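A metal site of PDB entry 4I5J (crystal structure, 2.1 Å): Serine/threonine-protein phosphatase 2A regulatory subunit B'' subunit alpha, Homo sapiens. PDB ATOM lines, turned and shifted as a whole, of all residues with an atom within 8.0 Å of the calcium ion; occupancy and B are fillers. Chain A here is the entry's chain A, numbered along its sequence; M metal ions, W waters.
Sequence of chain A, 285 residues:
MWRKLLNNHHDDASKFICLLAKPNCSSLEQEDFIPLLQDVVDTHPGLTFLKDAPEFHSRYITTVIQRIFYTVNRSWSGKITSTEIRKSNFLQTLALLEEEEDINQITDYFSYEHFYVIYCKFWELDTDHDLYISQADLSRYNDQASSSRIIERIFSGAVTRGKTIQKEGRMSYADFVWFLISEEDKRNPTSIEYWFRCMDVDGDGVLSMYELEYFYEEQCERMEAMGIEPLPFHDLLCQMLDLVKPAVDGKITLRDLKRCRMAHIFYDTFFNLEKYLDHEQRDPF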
ATOM      1  N   PHE A 196      -3.068   8.346   9.924  1.00  0.00           N
ATOM      2  CA  PHE A 196      -3.447   8.369   8.508  1.00  0.00           C
ATOM      3  C   PHE A 196      -3.274   6.983   7.905  1.00  0.00           C
ATOM      4  O   PHE A 196      -4.156   6.518   7.192  1.00  0.00           O
ATOM      5  CB  PHE A 196      -2.625   9.387   7.725  1.00  0.00           C
ATOM      6  CG  PHE A 196      -3.053   9.510   6.294  1.00  0.00           C
ATOM      7  CD1 PHE A 196      -3.976  10.486   5.919  1.00  0.00           C
ATOM      8  CD2 PHE A 196      -2.560   8.643   5.328  1.00  0.00           C
ATOM      9  CE1 PHE A 196      -4.380  10.604   4.602  1.00  0.00           C
ATOM     10  CE2 PHE A 196      -2.987   8.740   4.006  1.00  0.00           C
ATOM     11  CZ  PHE A 196      -3.887   9.724   3.633  1.00  0.00           C
ATOM     12  N   MET A 199      -6.123   4.834   8.995  1.00  0.00           N
ATOM     13  CA  MET A 199      -7.382   5.170   8.327  1.00  0.00           C
ATOM     14  C   MET A 199      -7.369   4.883   6.835  1.00  0.00           C
ATOM     15  O   MET A 199      -8.423   4.628   6.239  1.00  0.00           O
ATOM     16  CB  MET A 199      -7.764   6.632   8.560  1.00  0.00           C
ATOM     17  CG  MET A 199      -8.146   6.918  10.016  1.00  0.00           C
ATOM     18  SD  MET A 199      -8.986   8.510  10.204  1.00  0.00           S
ATOM     19  CE  MET A 199     -10.512   8.136   9.313  1.00  0.00           C
ATOM     20  N   ASP A 200      -6.191   4.891   6.230  1.00  0.00           N
ATOM     21  CA  ASP A 200      -6.087   4.594   4.804  1.00  0.00           C
ATOM     22  C   ASP A 200      -6.219   3.095   4.566  1.00  0.00           C
ATOM     23  O   ASP A 200      -5.249   2.424   4.230  1.00  0.00           O
ATOM     24  CB  ASP A 200      -4.768   5.118   4.223  1.00  0.00           C
ATOM     25  CG  ASP A 200      -4.704   5.006   2.718  1.00  0.00           C
ATOM     26  OD1 ASP A 200      -5.726   4.685   2.099  1.00  0.00           O
ATOM     27  OD2 ASP A 200      -3.622   5.231   2.144  1.00  0.00           O
ATOM     28  N   VAL A 201      -7.430   2.580   4.764  1.00  0.00           N
ATOM     29  CA  VAL A 201      -7.651   1.134   4.706  1.00  0.00           C
ATOM     30  C   VAL A 201      -7.049   0.454   3.477  1.00  0.00           C
ATOM     31  O   VAL A 201      -6.326  -0.539   3.615  1.00  0.00           O
ATOM     32  CB  VAL A 201      -9.143   0.802   4.755  1.00  0.00           C
ATOM     33  CG1 VAL A 201      -9.365  -0.717   4.619  1.00  0.00           C
ATOM     34  CG2 VAL A 201      -9.762   1.337   6.045  1.00  0.00           C
ATOM     35  N   ASP A 202      -7.310   0.984   2.282  1.00  0.00           N
ATOM     36  CA  ASP A 202      -6.841   0.343   1.054  1.00  0.00           C
ATOM     37  C   ASP A 202      -5.400   0.740   0.711  1.00  0.00           C
ATOM     38  O   ASP A 202      -4.827   0.255  -0.260  1.00  0.00           O
ATOM     39  CB  ASP A 202      -7.783   0.624  -0.128  1.00  0.00           C
ATOM     40  CG  ASP A 202      -7.883   2.114  -0.470  1.00  0.00           C
ATOM     41  OD1 ASP A 202      -7.034   2.912  -0.031  1.00  0.00           O
ATOM     42  OD2 ASP A 202      -8.845   2.508  -1.176  1.00  0.00           O
ATOM     43  N   GLY A 203      -4.843   1.664   1.482  1.00  0.00           N
ATOM     44  CA  GLY A 203      -3.455   2.074   1.311  1.00  0.00           C
ATOM     45  C   GLY A 203      -3.102   2.832   0.039  1.00  0.00           C
ATOM     46  O   GLY A 203      -1.936   2.851  -0.357  1.00  0.00           O
ATOM     47  N   ASP A 204      -4.079   3.490  -0.584  1.00  0.00           N
ATOM     48  CA  ASP A 204      -3.807   4.227  -1.818  1.00  0.00           C
ATOM     49  C   ASP A 204      -3.288   5.642  -1.600  1.00  0.00           C
ATOM     50  O   ASP A 204      -3.086   6.380  -2.552  1.00  0.00           O
ATOM     51  CB  ASP A 204      -5.032   4.251  -2.745  1.00  0.00           C
ATOM     52  CG  ASP A 204      -6.234   4.984  -2.128  1.00  0.00           C
ATOM     53  OD1 ASP A 204      -6.160   5.430  -0.953  1.00  0.00           O
ATOM     54  OD2 ASP A 204      -7.275   5.096  -2.837  1.00  0.00           O
ATOM     55  N   GLY A 205      -3.074   6.041  -0.351  1.00  0.00           N
ATOM     56  CA  GLY A 205      -2.511   7.353  -0.081  1.00  0.00           C
ATOM     57  C   GLY A 205      -3.557   8.446   0.123  1.00  0.00           C
ATOM     58  O   GLY A 205      -3.203   9.586   0.374  1.00  0.00           O
ATOM     59  N   VAL A 206      -4.842   8.123  -0.006  1.00  0.00           N
ATOM     60  CA  VAL A 206      -5.888   9.091   0.315  1.00  0.00           C
ATOM     61  C   VAL A 206      -6.993   8.458   1.136  1.00  0.00           C
ATOM     62  O   VAL A 206      -7.183   7.242   1.079  1.00  0.00           O
ATOM     63  CB  VAL A 206      -6.541   9.672  -0.948  1.00  0.00           C
ATOM     64  CG1 VAL A 206      -5.467  10.169  -1.931  1.00  0.00           C
ATOM     65  CG2 VAL A 206      -7.462   8.638  -1.591  1.00  0.00           C
ATOM     66  N   LEU A 207      -7.729   9.270   1.889  1.00  0.00           N
ATOM     67  CA  LEU A 207      -8.867   8.810   2.672  1.00  0.00           C
ATOM     68  C   LEU A 207     -10.093   9.099   1.843  1.00  0.00           C
ATOM     69  O   LEU A 207     -10.401  10.253   1.587  1.00  0.00           O
ATOM     70  CB  LEU A 207      -8.937   9.539   4.016  1.00  0.00           C
ATOM     71  CG  LEU A 207      -7.659   9.426   4.854  1.00  0.00           C
ATOM     72  CD1 LEU A 207      -7.865  10.012   6.242  1.00  0.00           C
ATOM     73  CD2 LEU A 207      -7.194   7.977   4.930  1.00  0.00           C
ATOM     74  N   SER A 208     -10.758   8.043   1.374  1.00  0.00           N
ATOM     75  CA  SER A 208     -11.966   8.184   0.575  1.00  0.00           C
ATOM     76  C   SER A 208     -13.148   8.275   1.538  1.00  0.00           C
ATOM     77  O   SER A 208     -13.014   7.969   2.736  1.00  0.00           O
ATOM     78  CB  SER A 208     -12.120   6.984  -0.338  1.00  0.00           C
ATOM     79  OG  SER A 208     -12.203   5.792   0.444  1.00  0.00           O
ATOM     80  N   MET A 209     -14.313   8.671   1.023  1.00  0.00           N
ATOM     81  CA  MET A 209     -15.451   8.894   1.894  1.00  0.00           C
ATOM     82  C   MET A 209     -15.981   7.585   2.449  1.00  0.00           C
ATOM     83  O   MET A 209     -16.607   7.566   3.516  1.00  0.00           O
ATOM     84  CB  MET A 209     -16.565   9.643   1.172  1.00  0.00           C
ATOM     85  CG  MET A 209     -16.195  11.061   0.803  1.00  0.00           C
ATOM     86  SD  MET A 209     -17.522  11.801  -0.182  1.00  0.00           S
ATOM     87  CE  MET A 209     -16.809  13.404  -0.611  1.00  0.00           C
ATOM     88  N   TYR A 210     -15.726   6.490   1.745  1.00  0.00           N
ATOM     89  CA  TYR A 210     -16.177   5.202   2.241  1.00  0.00           C
ATOM     90  C   TYR A 210     -15.234   4.639   3.306  1.00  0.00           C
ATOM     91  O   TYR A 210     -15.643   3.827   4.113  1.00  0.00           O
ATOM     92  CB  TYR A 210     -16.419   4.193   1.101  1.00  0.00           C
ATOM     93  CG  TYR A 210     -15.292   4.065   0.111  1.00  0.00           C
ATOM     94  CD1 TYR A 210     -14.317   3.100   0.285  1.00  0.00           C
ATOM     95  CD2 TYR A 210     -15.228   4.887  -1.012  1.00  0.00           C
ATOM     96  CE1 TYR A 210     -13.292   2.961  -0.607  1.00  0.00           C
ATOM     97  CE2 TYR A 210     -14.188   4.761  -1.920  1.00  0.00           C
ATOM     98  CZ  TYR A 210     -13.229   3.786  -1.716  1.00  0.00           C
ATOM     99  OH  TYR A 210     -12.188   3.637  -2.597  1.00  0.00           O
ATOM    100  N   GLU A 211     -13.980   5.083   3.299  1.00  0.00           N
ATOM    101  CA  GLU A 211     -13.074   4.730   4.397  1.00  0.00           C
ATOM    102  C   GLU A 211     -13.501   5.517   5.633  1.00  0.00           C
ATOM    103  O   GLU A 211     -13.588   4.962   6.726  1.00  0.00           O
ATOM    104  CB  GLU A 211     -11.612   4.981   4.025  1.00  0.00           C
ATOM    105  CG  GLU A 211     -11.087   3.938   3.061  1.00  0.00           C
ATOM    106  CD  GLU A 211      -9.772   4.313   2.382  1.00  0.00           C
ATOM    107  OE1 GLU A 211      -9.471   5.525   2.273  1.00  0.00           O
ATOM    108  OE2 GLU A 211      -9.046   3.385   1.941  1.00  0.00           O
ATOM    109  N   LEU A 212     -13.800   6.798   5.444  1.00  0.00           N
ATOM    110  CA  LEU A 212     -14.376   7.580   6.535  1.00  0.00           C
ATOM    111  C   LEU A 212     -15.656   6.938   7.120  1.00  0.00           C
ATOM    112  O   LEU A 212     -15.811   6.870   8.353  1.00  0.00           O
ATOM    113  CB  LEU A 212     -14.643   9.020   6.093  1.00  0.00           C
ATOM    114  CG  LEU A 212     -13.401   9.843   5.709  1.00  0.00           C
ATOM    115  CD1 LEU A 212     -13.749  11.312   5.505  1.00  0.00           C
ATOM    116  CD2 LEU A 212     -12.342   9.718   6.732  1.00  0.00           C
ATOM    117  N   GLY A 250     -13.159  13.974  -1.819  1.00  0.00           N
ATOM    118  CA  GLY A 250     -13.336  12.542  -1.698  1.00  0.00           C
ATOM    119  C   GLY A 250     -12.006  11.831  -1.665  1.00  0.00           C
ATOM    120  O   GLY A 250     -11.948  10.614  -1.738  1.00  0.00           O
ATOM    121  N   LYS A 251     -10.926  12.597  -1.582  1.00  0.00           N
ATOM    122  CA  LYS A 251      -9.560  12.045  -1.581  1.00  0.00           C
ATOM    123  C   LYS A 251      -8.661  12.855  -0.640  1.00  0.00           C
ATOM    124  O   LYS A 251      -7.787  13.599  -1.072  1.00  0.00           O
ATOM    125  CB  LYS A 251      -8.982  11.978  -3.009  1.00  0.00           C
ATOM    126  CG  LYS A 251      -9.830  11.126  -3.977  1.00  0.00           C
ATOM    127  CD  LYS A 251      -9.370  11.224  -5.424  1.00  0.00           C
ATOM    128  CE  LYS A 251      -7.966  10.721  -5.605  1.00  0.00           C
ATOM    129  NZ  LYS A 251      -7.882   9.258  -5.352  1.00  0.00           N
ATOM    130  N   ILE A 252      -8.902  12.735   0.660  1.00  0.00           N
ATOM    131  CA  ILE A 252      -8.139  13.490   1.646  1.00  0.00           C
ATOM    132  C   ILE A 252      -6.719  12.967   1.802  1.00  0.00           C
ATOM    133  O   ILE A 252      -6.525  11.772   2.037  1.00  0.00           O
ATOM    134  CB  ILE A 252      -8.845  13.471   3.025  1.00  0.00           C
ATOM    135  CG1 ILE A 252     -10.175  14.222   2.909  1.00  0.00           C
ATOM    136  CG2 ILE A 252      -7.976  14.108   4.120  1.00  0.00           C
ATOM    137  CD1 ILE A 252     -11.115  13.932   4.032  1.00  0.00           C
HETATM  138 CA    CA M   1      -7.599   4.997   0.829  1.00  0.00          CA
HETATM  139  O   HOH W   1      -9.274   5.022  -0.910  1.00  0.00           O
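Water W1 lies within hydrogen-bond range of OD2 of Asp 202 (2.6 Å), OD2 of Asp 204 (2.8 Å) and OG of Ser 208 (3.3 Å).
The backbone NH (N) of Gly 203 sits close to the side-chain carboxylate (OD1) of Asp 200 (3.2 Å).
The side-chain carboxylate of Asp 200 sits at hydrogen-bond distance from the backbone NH of Gly 205.
The side-chain carboxylate (OE2) of Glu 211 lies close to the backbone NH (N) of Val 201.
N of Glu 211 sits close to OG of Ser 208 (3.4 Å).
The calcium ion is bound by OD1 of Asp 200, 2.3 Å away.
The calcium ion is bound by O of Val 206 (2.3 Å).
The calcium ion is bound by OD1 of Asp 202 (2.3 Å).
OD1 of Asp 204 is bound to the calcium ion, at 2.3 Å.
The calcium ion is bound by water W1.
The side-chain carboxylate (OE1) of Glu 211 is bound to the calcium ion.
The side-chain carboxylate (OE2) of Glu 211 is bound to the calcium ion.
The calcium ion has seven donor atoms within binding distance.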
